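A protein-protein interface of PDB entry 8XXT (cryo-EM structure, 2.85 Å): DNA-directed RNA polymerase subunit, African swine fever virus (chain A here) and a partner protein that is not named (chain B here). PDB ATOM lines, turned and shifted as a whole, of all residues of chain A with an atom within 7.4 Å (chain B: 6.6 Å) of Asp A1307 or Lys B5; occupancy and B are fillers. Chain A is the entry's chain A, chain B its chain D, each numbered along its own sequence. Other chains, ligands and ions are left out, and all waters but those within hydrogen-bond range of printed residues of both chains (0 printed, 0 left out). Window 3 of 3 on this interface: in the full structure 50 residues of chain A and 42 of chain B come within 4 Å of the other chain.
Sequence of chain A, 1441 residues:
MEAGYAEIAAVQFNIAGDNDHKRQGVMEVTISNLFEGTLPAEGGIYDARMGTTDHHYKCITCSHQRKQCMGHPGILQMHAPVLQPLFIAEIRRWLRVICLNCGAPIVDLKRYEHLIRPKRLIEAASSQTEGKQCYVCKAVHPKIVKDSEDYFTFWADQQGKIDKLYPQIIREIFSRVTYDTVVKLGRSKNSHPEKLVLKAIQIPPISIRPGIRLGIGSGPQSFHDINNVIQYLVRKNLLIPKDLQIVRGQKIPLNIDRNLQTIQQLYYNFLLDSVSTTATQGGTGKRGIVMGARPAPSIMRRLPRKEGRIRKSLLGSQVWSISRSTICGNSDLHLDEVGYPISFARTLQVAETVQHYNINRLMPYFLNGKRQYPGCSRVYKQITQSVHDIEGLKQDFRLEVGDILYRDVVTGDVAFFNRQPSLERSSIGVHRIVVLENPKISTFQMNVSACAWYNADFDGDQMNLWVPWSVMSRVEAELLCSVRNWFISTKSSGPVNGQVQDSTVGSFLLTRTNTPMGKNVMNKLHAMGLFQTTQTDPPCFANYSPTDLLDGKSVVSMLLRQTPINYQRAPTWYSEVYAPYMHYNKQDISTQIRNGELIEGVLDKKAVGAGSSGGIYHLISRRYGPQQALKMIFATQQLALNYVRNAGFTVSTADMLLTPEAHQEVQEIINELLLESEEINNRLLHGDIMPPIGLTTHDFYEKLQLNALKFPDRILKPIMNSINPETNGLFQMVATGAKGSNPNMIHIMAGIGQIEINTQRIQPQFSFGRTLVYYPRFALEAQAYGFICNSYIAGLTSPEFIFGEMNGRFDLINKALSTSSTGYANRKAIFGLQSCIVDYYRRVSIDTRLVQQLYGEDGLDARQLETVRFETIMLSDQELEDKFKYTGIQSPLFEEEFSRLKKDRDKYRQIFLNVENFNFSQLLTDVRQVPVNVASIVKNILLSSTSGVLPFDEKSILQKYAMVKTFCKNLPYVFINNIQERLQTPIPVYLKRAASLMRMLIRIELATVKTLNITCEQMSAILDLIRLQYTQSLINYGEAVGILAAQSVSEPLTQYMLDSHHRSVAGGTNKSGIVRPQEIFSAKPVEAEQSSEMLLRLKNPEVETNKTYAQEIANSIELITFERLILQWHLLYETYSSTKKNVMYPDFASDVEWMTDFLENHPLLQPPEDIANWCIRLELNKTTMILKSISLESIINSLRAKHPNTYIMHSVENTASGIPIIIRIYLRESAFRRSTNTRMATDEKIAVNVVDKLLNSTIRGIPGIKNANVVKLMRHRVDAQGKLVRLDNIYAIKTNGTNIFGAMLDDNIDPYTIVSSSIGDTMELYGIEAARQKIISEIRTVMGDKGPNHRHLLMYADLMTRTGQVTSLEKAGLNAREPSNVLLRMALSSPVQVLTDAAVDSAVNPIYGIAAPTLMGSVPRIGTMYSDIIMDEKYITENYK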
ATOM      1  N   LEU A1098      -6.052  15.744  -0.719  1.00  0.00           N
ATOM      2  CA  LEU A1098      -7.210  16.192  -1.477  1.00  0.00           C
ATOM      3  C   LEU A1098      -8.099  15.008  -1.824  1.00  0.00           C
ATOM      4  O   LEU A1098      -7.614  13.958  -2.253  1.00  0.00           O
ATOM      5  CB  LEU A1098      -6.757  16.906  -2.747  1.00  0.00           C
ATOM      6  CG  LEU A1098      -6.001  18.211  -2.516  1.00  0.00           C
ATOM      7  CD1 LEU A1098      -5.054  18.496  -3.663  1.00  0.00           C
ATOM      8  CD2 LEU A1098      -6.989  19.344  -2.344  1.00  0.00           C
ATOM      9  N   LYS A1099      -9.404  15.177  -1.629  1.00  0.00           N
ATOM     10  CA  LYS A1099     -10.342  14.116  -1.959  1.00  0.00           C
ATOM     11  C   LYS A1099     -10.284  13.826  -3.453  1.00  0.00           C
ATOM     12  O   LYS A1099     -10.064  14.729  -4.264  1.00  0.00           O
ATOM     13  CB  LYS A1099     -11.757  14.507  -1.542  1.00  0.00           C
ATOM     14  CG  LYS A1099     -12.710  13.330  -1.435  1.00  0.00           C
ATOM     15  CD  LYS A1099     -14.110  13.779  -1.047  1.00  0.00           C
ATOM     16  CE  LYS A1099     -14.930  12.617  -0.512  1.00  0.00           C
ATOM     17  NZ  LYS A1099     -14.489  12.201   0.848  1.00  0.00           N
ATOM     18  N   ASN A1100     -10.459  12.547  -3.804  1.00  0.00           N
ATOM     19  CA  ASN A1100     -10.322  11.996  -5.150  1.00  0.00           C
ATOM     20  C   ASN A1100      -8.854  11.982  -5.559  1.00  0.00           C
ATOM     21  O   ASN A1100      -8.105  12.912  -5.235  1.00  0.00           O
ATOM     22  CB  ASN A1100     -11.157  12.782  -6.163  1.00  0.00           C
ATOM     23  CG  ASN A1100     -12.634  12.490  -6.046  1.00  0.00           C
ATOM     24  OD1 ASN A1100     -13.190  12.478  -4.950  1.00  0.00           O
ATOM     25  ND2 ASN A1100     -13.282  12.256  -7.181  1.00  0.00           N
ATOM     26  N   TYR A1109      -5.483  23.259  -8.866  1.00  0.00           N
ATOM     27  CA  TYR A1109      -6.563  22.888  -7.962  1.00  0.00           C
ATOM     28  C   TYR A1109      -6.052  22.696  -6.541  1.00  0.00           C
ATOM     29  O   TYR A1109      -6.807  22.885  -5.581  1.00  0.00           O
ATOM     30  CB  TYR A1109      -7.242  21.614  -8.455  1.00  0.00           C
ATOM     31  CG  TYR A1109      -8.240  21.043  -7.481  1.00  0.00           C
ATOM     32  CD1 TYR A1109      -9.409  21.724  -7.175  1.00  0.00           C
ATOM     33  CD2 TYR A1109      -8.005  19.832  -6.850  1.00  0.00           C
ATOM     34  CE1 TYR A1109     -10.326  21.204  -6.284  1.00  0.00           C
ATOM     35  CE2 TYR A1109      -8.908  19.311  -5.952  1.00  0.00           C
ATOM     36  CZ  TYR A1109     -10.069  19.997  -5.674  1.00  0.00           C
ATOM     37  OH  TYR A1109     -10.972  19.473  -4.778  1.00  0.00           O
ATOM     38  N   ILE A1113      -7.443  25.179  -3.076  1.00  0.00           N
ATOM     39  CA  ILE A1113      -8.049  24.538  -1.914  1.00  0.00           C
ATOM     40  C   ILE A1113      -7.245  24.843  -0.658  1.00  0.00           C
ATOM     41  O   ILE A1113      -7.814  24.991   0.431  1.00  0.00           O
ATOM     42  CB  ILE A1113      -8.193  23.022  -2.145  1.00  0.00           C
ATOM     43  CG1 ILE A1113      -9.080  22.757  -3.360  1.00  0.00           C
ATOM     44  CG2 ILE A1113      -8.763  22.336  -0.910  1.00  0.00           C
ATOM     45  CD1 ILE A1113     -10.539  22.543  -3.022  1.00  0.00           C
ATOM     46  N   PHE A1301     -10.204  17.899  13.726  1.00  0.00           N
ATOM     47  CA  PHE A1301     -11.663  17.924  13.699  1.00  0.00           C
ATOM     48  C   PHE A1301     -12.184  18.827  12.591  1.00  0.00           C
ATOM     49  O   PHE A1301     -13.135  18.470  11.886  1.00  0.00           O
ATOM     50  CB  PHE A1301     -12.202  18.378  15.054  1.00  0.00           C
ATOM     51  CG  PHE A1301     -13.698  18.408  15.128  1.00  0.00           C
ATOM     52  CD1 PHE A1301     -14.457  17.452  14.478  1.00  0.00           C
ATOM     53  CD2 PHE A1301     -14.348  19.391  15.851  1.00  0.00           C
ATOM     54  CE1 PHE A1301     -15.830  17.478  14.547  1.00  0.00           C
ATOM     55  CE2 PHE A1301     -15.724  19.418  15.922  1.00  0.00           C
ATOM     56  CZ  PHE A1301     -16.465  18.460  15.270  1.00  0.00           C
ATOM     57  N   GLY A1302     -11.577  20.001  12.418  1.00  0.00           N
ATOM     58  CA  GLY A1302     -12.012  20.892  11.357  1.00  0.00           C
ATOM     59  C   GLY A1302     -11.795  20.309   9.975  1.00  0.00           C
ATOM     60  O   GLY A1302     -12.660  20.416   9.103  1.00  0.00           O
ATOM     61  N   ALA A1303     -10.641  19.672   9.759  1.00  0.00           N
ATOM     62  CA  ALA A1303     -10.346  19.102   8.450  1.00  0.00           C
ATOM     63  C   ALA A1303     -11.341  18.012   8.084  1.00  0.00           C
ATOM     64  O   ALA A1303     -11.722  17.876   6.918  1.00  0.00           O
ATOM     65  CB  ALA A1303      -8.919  18.562   8.423  1.00  0.00           C
ATOM     66  N   MET A1304     -11.771  17.221   9.069  1.00  0.00           N
ATOM     67  CA  MET A1304     -12.805  16.223   8.811  1.00  0.00           C
ATOM     68  C   MET A1304     -14.101  16.882   8.364  1.00  0.00           C
ATOM     69  O   MET A1304     -14.823  16.340   7.518  1.00  0.00           O
ATOM     70  CB  MET A1304     -13.042  15.379  10.059  1.00  0.00           C
ATOM     71  CG  MET A1304     -11.774  14.907  10.729  1.00  0.00           C
ATOM     72  SD  MET A1304     -11.912  13.262  11.427  1.00  0.00           S
ATOM     73  CE  MET A1304     -12.645  13.663  13.007  1.00  0.00           C
ATOM     74  N   LEU A1305     -14.420  18.049   8.931  1.00  0.00           N
ATOM     75  CA  LEU A1305     -15.606  18.780   8.500  1.00  0.00           C
ATOM     76  C   LEU A1305     -15.485  19.209   7.045  1.00  0.00           C
ATOM     77  O   LEU A1305     -16.467  19.172   6.295  1.00  0.00           O
ATOM     78  CB  LEU A1305     -15.833  19.992   9.402  1.00  0.00           C
ATOM     79  CG  LEU A1305     -15.984  19.725  10.899  1.00  0.00           C
ATOM     80  CD1 LEU A1305     -16.488  20.970  11.609  1.00  0.00           C
ATOM     81  CD2 LEU A1305     -16.900  18.542  11.155  1.00  0.00           C
ATOM     82  N   ASP A1306     -14.290  19.617   6.632  1.00  0.00           N
ATOM     83  CA  ASP A1306     -14.058  20.066   5.266  1.00  0.00           C
ATOM     84  C   ASP A1306     -14.275  18.918   4.286  1.00  0.00           C
ATOM     85  O   ASP A1306     -13.651  17.860   4.411  1.00  0.00           O
ATOM     86  CB  ASP A1306     -12.643  20.621   5.151  1.00  0.00           C
ATOM     87  CG  ASP A1306     -12.493  21.586   4.011  1.00  0.00           C
ATOM     88  OD1 ASP A1306     -12.871  21.223   2.882  1.00  0.00           O
ATOM     89  OD2 ASP A1306     -12.013  22.714   4.245  1.00  0.00           O
ATOM     90  N   ASP A1307     -15.163  19.124   3.310  1.00  0.00           N
ATOM     91  CA  ASP A1307     -15.497  18.064   2.367  1.00  0.00           C
ATOM     92  C   ASP A1307     -14.564  18.009   1.164  1.00  0.00           C
ATOM     93  O   ASP A1307     -14.565  17.001   0.449  1.00  0.00           O
ATOM     94  CB  ASP A1307     -16.942  18.216   1.888  1.00  0.00           C
ATOM     95  CG  ASP A1307     -17.924  17.424   2.736  1.00  0.00           C
ATOM     96  OD1 ASP A1307     -18.023  16.194   2.544  1.00  0.00           O
ATOM     97  OD2 ASP A1307     -18.592  18.032   3.599  1.00  0.00           O
ATOM     98  N   ASN A1308     -13.775  19.055   0.913  1.00  0.00           N
ATOM     99  CA  ASN A1308     -12.790  18.979  -0.161  1.00  0.00           C
ATOM    100  C   ASN A1308     -11.536  18.226   0.258  1.00  0.00           C
ATOM    101  O   ASN A1308     -10.651  18.011  -0.576  1.00  0.00           O
ATOM    102  CB  ASN A1308     -12.416  20.376  -0.660  1.00  0.00           C
ATOM    103  CG  ASN A1308     -13.534  21.376  -0.486  1.00  0.00           C
ATOM    104  OD1 ASN A1308     -13.571  22.128   0.484  1.00  0.00           O
ATOM    105  ND2 ASN A1308     -14.457  21.391  -1.436  1.00  0.00           N
ATOM    106  N   ILE A1309     -11.440  17.826   1.522  1.00  0.00           N
ATOM    107  CA  ILE A1309     -10.277  17.133   2.058  1.00  0.00           C
ATOM    108  C   ILE A1309     -10.701  15.748   2.518  1.00  0.00           C
ATOM    109  O   ILE A1309     -11.707  15.601   3.221  1.00  0.00           O
ATOM    110  CB  ILE A1309      -9.642  17.922   3.215  1.00  0.00           C
ATOM    111  CG1 ILE A1309      -9.076  19.241   2.701  1.00  0.00           C
ATOM    112  CG2 ILE A1309      -8.565  17.102   3.877  1.00  0.00           C
ATOM    113  CD1 ILE A1309      -8.237  19.089   1.460  1.00  0.00           C
ATOM    114  N   ASP A1310      -9.934  14.738   2.126  1.00  0.00           N
ATOM    115  CA  ASP A1310     -10.204  13.369   2.533  1.00  0.00           C
ATOM    116  C   ASP A1310     -10.064  13.244   4.046  1.00  0.00           C
ATOM    117  O   ASP A1310      -8.992  13.548   4.589  1.00  0.00           O
ATOM    118  CB  ASP A1310      -9.243  12.415   1.832  1.00  0.00           C
ATOM    119  CG  ASP A1310      -9.669  10.970   1.945  1.00  0.00           C
ATOM    120  OD1 ASP A1310     -10.889  10.711   1.966  1.00  0.00           O
ATOM    121  OD2 ASP A1310      -8.786  10.090   2.003  1.00  0.00           O
ATOM    122  N   PRO A1311     -11.105  12.805   4.760  1.00  0.00           N
ATOM    123  CA  PRO A1311     -11.017  12.754   6.225  1.00  0.00           C
ATOM    124  C   PRO A1311     -10.258  11.557   6.763  1.00  0.00           C
ATOM    125  O   PRO A1311      -9.790  11.610   7.908  1.00  0.00           O
ATOM    126  CB  PRO A1311     -12.486  12.699   6.654  1.00  0.00           C
ATOM    127  CG  PRO A1311     -13.150  11.969   5.531  1.00  0.00           C
ATOM    128  CD  PRO A1311     -12.430  12.389   4.272  1.00  0.00           C
ATOM    129  N   MET B   1     -20.976  21.041   7.133  1.00  0.00           N
ATOM    130  CA  MET B   1     -20.869  21.542   8.498  1.00  0.00           C
ATOM    131  C   MET B   1     -20.986  20.328   9.420  1.00  0.00           C
ATOM    132  O   MET B   1     -21.363  19.248   8.966  1.00  0.00           O
ATOM    133  CB  MET B   1     -21.943  22.612   8.756  1.00  0.00           C
ATOM    134  CG  MET B   1     -21.644  23.614   9.875  1.00  0.00           C
ATOM    135  SD  MET B   1     -22.931  23.859  11.119  1.00  0.00           S
ATOM    136  CE  MET B   1     -23.003  22.277  11.931  1.00  0.00           C
ATOM    137  N   ALA B   2     -20.652  20.502  10.701  1.00  0.00           N
ATOM    138  CA  ALA B   2     -20.487  19.356  11.592  1.00  0.00           C
ATOM    139  C   ALA B   2     -21.756  18.518  11.688  1.00  0.00           C
ATOM    140  O   ALA B   2     -21.693  17.283  11.708  1.00  0.00           O
ATOM    141  CB  ALA B   2     -20.061  19.833  12.980  1.00  0.00           C
ATOM    142  N   MET B   3     -22.917  19.172  11.740  1.00  0.00           N
ATOM    143  CA  MET B   3     -24.160  18.455  12.003  1.00  0.00           C
ATOM    144  C   MET B   3     -24.534  17.523  10.858  1.00  0.00           C
ATOM    145  O   MET B   3     -25.137  16.474  11.093  1.00  0.00           O
ATOM    146  CB  MET B   3     -25.289  19.448  12.280  1.00  0.00           C
ATOM    147  CG  MET B   3     -26.250  19.027  13.392  1.00  0.00           C
ATOM    148  SD  MET B   3     -25.611  18.858  15.079  1.00  0.00           S
ATOM    149  CE  MET B   3     -24.153  19.902  15.076  1.00  0.00           C
ATOM    150  N   GLN B   4     -24.194  17.879   9.618  1.00  0.00           N
ATOM    151  CA  GLN B   4     -24.416  16.962   8.503  1.00  0.00           C
ATOM    152  C   GLN B   4     -23.566  15.704   8.674  1.00  0.00           C
ATOM    153  O   GLN B   4     -24.043  14.575   8.481  1.00  0.00           O
ATOM    154  CB  GLN B   4     -24.082  17.683   7.192  1.00  0.00           C
ATOM    155  CG  GLN B   4     -24.241  16.962   5.828  1.00  0.00           C
ATOM    156  CD  GLN B   4     -25.384  15.953   5.718  1.00  0.00           C
ATOM    157  OE1 GLN B   4     -25.486  14.992   6.471  1.00  0.00           O
ATOM    158  NE2 GLN B   4     -26.259  16.185   4.747  1.00  0.00           N
ATOM    159  N   LYS B   5     -22.303  15.881   9.070  1.00  0.00           N
ATOM    160  CA  LYS B   5     -21.442  14.729   9.305  1.00  0.00           C
ATOM    161  C   LYS B   5     -21.979  13.859  10.429  1.00  0.00           C
ATOM    162  O   LYS B   5     -21.924  12.629  10.346  1.00  0.00           O
ATOM    163  CB  LYS B   5     -20.015  15.183   9.601  1.00  0.00           C
ATOM    164  CG  LYS B   5     -19.646  16.476   8.925  1.00  0.00           C
ATOM    165  CD  LYS B   5     -18.193  16.455   8.527  1.00  0.00           C
ATOM    166  CE  LYS B   5     -17.928  15.378   7.494  1.00  0.00           C
ATOM    167  NZ  LYS B   5     -18.670  15.617   6.229  1.00  0.00           N
ATOM    168  N   LEU B   6     -22.495  14.474  11.495  1.00  0.00           N
ATOM    169  CA  LEU B   6     -23.177  13.679  12.511  1.00  0.00           C
ATOM    170  C   LEU B   6     -24.369  12.947  11.915  1.00  0.00           C
ATOM    171  O   LEU B   6     -24.559  11.754  12.165  1.00  0.00           O
ATOM    172  CB  LEU B   6     -23.622  14.556  13.679  1.00  0.00           C
ATOM    173  CG  LEU B   6     -22.601  14.819  14.784  1.00  0.00           C
ATOM    174  CD1 LEU B   6     -21.907  16.147  14.587  1.00  0.00           C
ATOM    175  CD2 LEU B   6     -23.273  14.758  16.143  1.00  0.00           C
ATOM    176  N   PHE B   7     -25.159  13.637  11.093  1.00  0.00           N
ATOM    177  CA  PHE B   7     -26.375  13.056  10.538  1.00  0.00           C
ATOM    178  C   PHE B   7     -26.085  11.860   9.643  1.00  0.00           C
ATOM    179  O   PHE B   7     -26.966  11.027   9.419  1.00  0.00           O
ATOM    180  CB  PHE B   7     -27.144  14.123   9.758  1.00  0.00           C
ATOM    181  CG  PHE B   7     -28.381  13.607   9.086  1.00  0.00           C
ATOM    182  CD1 PHE B   7     -29.363  12.960   9.814  1.00  0.00           C
ATOM    183  CD2 PHE B   7     -28.555  13.760   7.723  1.00  0.00           C
ATOM    184  CE1 PHE B   7     -30.495  12.482   9.194  1.00  0.00           C
ATOM    185  CE2 PHE B   7     -29.685  13.283   7.099  1.00  0.00           C
ATOM    186  CZ  PHE B   7     -30.653  12.645   7.835  1.00  0.00           C
ATOM    187  N   THR B   8     -24.883  11.771   9.088  1.00  0.00           N
ATOM    188  CA  THR B   8     -24.585  10.560   8.324  1.00  0.00           C
ATOM    189  C   THR B   8     -23.862   9.509   9.171  1.00  0.00           C
ATOM    190  O   THR B   8     -24.228   8.322   9.172  1.00  0.00           O
ATOM    191  CB  THR B   8     -23.766  10.898   7.072  1.00  0.00           C
ATOM    192  OG1 THR B   8     -23.232   9.693   6.510  1.00  0.00           O
ATOM    193  CG2 THR B   8     -22.630  11.854   7.393  1.00  0.00           C
ATOM    194  N   TYR B   9     -22.845   9.926   9.918  1.00  0.00           N
ATOM    195  CA  TYR B   9     -22.009   8.969  10.616  1.00  0.00           C
ATOM    196  C   TYR B   9     -22.646   8.426  11.885  1.00  0.00           C
ATOM    197  O   TYR B   9     -22.175   7.410  12.391  1.00  0.00           O
ATOM    198  CB  TYR B   9     -20.656   9.604  10.917  1.00  0.00           C
ATOM    199  CG  TYR B   9     -19.873   9.911   9.663  1.00  0.00           C
ATOM    200  CD1 TYR B   9     -19.650   8.931   8.706  1.00  0.00           C
ATOM    201  CD2 TYR B   9     -19.377  11.181   9.424  1.00  0.00           C
ATOM    202  CE1 TYR B   9     -18.941   9.209   7.553  1.00  0.00           C
ATOM    203  CE2 TYR B   9     -18.665  11.466   8.277  1.00  0.00           C
ATOM    204  CZ  TYR B   9     -18.451  10.478   7.345  1.00  0.00           C
ATOM    205  OH  TYR B   9     -17.745  10.762   6.202  1.00  0.00           O
ATOM    206  N   ILE B  10     -23.724   9.026  12.392  1.00  0.00           N
ATOM    207  CA  ILE B  10     -24.409   8.398  13.514  1.00  0.00           C
ATOM    208  C   ILE B  10     -25.184   7.168  13.054  1.00  0.00           C
ATOM    209  O   ILE B  10     -25.248   6.167  13.775  1.00  0.00           O
ATOM    210  CB  ILE B  10     -25.304   9.407  14.255  1.00  0.00           C
ATOM    211  CG1 ILE B  10     -25.602   8.901  15.666  1.00  0.00           C
ATOM    212  CG2 ILE B  10     -26.594   9.668  13.509  1.00  0.00           C
ATOM    213  CD1 ILE B  10     -24.379   8.802  16.546  1.00  0.00           C
ATOM    214  N   TYR B  28     -32.275  15.537   5.959  1.00  0.00           N
ATOM    215  CA  TYR B  28     -31.329  16.439   6.610  1.00  0.00           C
ATOM    216  C   TYR B  28     -32.009  17.727   7.062  1.00  0.00           C
ATOM    217  O   TYR B  28     -31.726  18.229   8.156  1.00  0.00           O
ATOM    218  CB  TYR B  28     -30.166  16.750   5.665  1.00  0.00           C
ATOM    219  CG  TYR B  28     -29.191  17.796   6.170  1.00  0.00           C
ATOM    220  CD1 TYR B  28     -28.854  17.876   7.515  1.00  0.00           C
ATOM    221  CD2 TYR B  28     -28.620  18.712   5.301  1.00  0.00           C
ATOM    222  CE1 TYR B  28     -27.975  18.831   7.975  1.00  0.00           C
ATOM    223  CE2 TYR B  28     -27.738  19.673   5.752  1.00  0.00           C
ATOM    224  CZ  TYR B  28     -27.418  19.727   7.091  1.00  0.00           C
ATOM    225  OH  TYR B  28     -26.538  20.683   7.544  1.00  0.00           O
ATOM    226  N   PHE B 126     -18.146  11.284  16.105  1.00  0.00           N
ATOM    227  CA  PHE B 126     -19.105  10.820  15.109  1.00  0.00           C
ATOM    228  C   PHE B 126     -19.127  11.700  13.864  1.00  0.00           C
ATOM    229  O   PHE B 126     -20.146  11.749  13.171  1.00  0.00           O
ATOM    230  CB  PHE B 126     -20.515  10.734  15.697  1.00  0.00           C
ATOM    231  CG  PHE B 126     -20.596  10.005  17.003  1.00  0.00           C
ATOM    232  CD1 PHE B 126     -20.812   8.639  17.033  1.00  0.00           C
ATOM    233  CD2 PHE B 126     -20.479  10.684  18.202  1.00  0.00           C
ATOM    234  CE1 PHE B 126     -20.900   7.962  18.233  1.00  0.00           C
ATOM    235  CE2 PHE B 126     -20.564  10.011  19.404  1.00  0.00           C
ATOM    236  CZ  PHE B 126     -20.780   8.650  19.420  1.00  0.00           C
ATOM    237  N   CYS B 127     -18.036  12.399  13.561  1.00  0.00           N
ATOM    238  CA  CYS B 127     -17.936  13.173  12.331  1.00  0.00           C
ATOM    239  C   CYS B 127     -17.046  12.504  11.292  1.00  0.00           C
ATOM    240  O   CYS B 127     -16.536  13.182  10.394  1.00  0.00           O
ATOM    241  CB  CYS B 127     -17.442  14.587  12.625  1.00  0.00           C
ATOM    242  SG  CYS B 127     -18.435  15.457  13.848  1.00  0.00           S
ATOM    243  N   ILE B 128     -16.852  11.190  11.397  1.00  0.00           N
ATOM    244  CA  ILE B 128     -16.056  10.434  10.440  1.00  0.00           C
ATOM    245  C   ILE B 128     -16.351   8.962  10.682  1.00  0.00           C
ATOM    246  O   ILE B 128     -16.696   8.570  11.802  1.00  0.00           O
ATOM    247  CB  ILE B 128     -14.559  10.745  10.601  1.00  0.00           C
ATOM    248  CG1 ILE B 128     -13.690   9.739   9.853  1.00  0.00           C
ATOM    249  CG2 ILE B 128     -14.192  10.673  12.060  1.00  0.00           C
ATOM    250  CD1 ILE B 128     -12.321  10.274   9.517  1.00  0.00           C
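OD2 of Asp A1307 lies within salt-bridge range of NZ of Lys B5 (3.6 Å).
Among the printed residues, merely in contact across the chains: Phe A1301 with Cys B127 (3.4 Å), Met A1304 with Lys B5 (3.3 Å), Met A1304 with Ile B128 (3.5 Å), Leu A1305 with Ala B2 (3.7 Å), Leu A1305 with Lys B5 (3.5 Å) and Pro A1311 with Ile B128 (3.3 Å).
Of chain B, only Lys B5 comes within 4 Å of Asp A1307. Of chain A, only Met A1304 (3.3 Å), Leu A1305 (3.5 Å) and Asp A1307 (3.6 Å) come within 4 Å of Lys B5. Of the printed residues of chain B, Phe A1301 touches Cys B127 (3.4 Å). Printed residues of chain A within 4 Å of Ile B128: Met A1304 (3.5 Å) and Pro A1311 (3.3 Å). Of the printed residues of chain B, Leu A1305 touches Ala B2 (3.7 Å) and Lys B5 (3.5 Å). Printed residues of chain B within 4 Å of Met A1304: Lys B5 (3.3 Å) and Ile B128 (3.5 Å). Of the printed residues of chain B, Pro A1311 touches Ile B128 (3.3 Å). Asn A1308 touches none of the printed residues of chain B. Tyr A1109 touches none of the printed residues of chain B. The nearest residue of chain B that does not touch Asp A1307 is Met B1 (5.2 Å). The nearest residue of chain A that does not touch Lys B5 is Asp A1306 (5.4 Å).
Of the 14 printed residues of chain B, 4 touch a printed residue of chain A. Hydrophobic or aromatic side chains of chain B that line the printed part of chain A: Ala B2 and Ile B128. Printed residues of chain A that touch a printed residue of chain B: Phe A1301, Met A1304, Leu A1305, Asp A1307 and Pro A1311. Hydrophobic or aromatic side chains of chain A within 4 Å of the printed part of chain B: Phe A1301, Met A1304, Leu A1305 and Pro A1311. Among the printed residues, 7 pairs touch across the chains.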
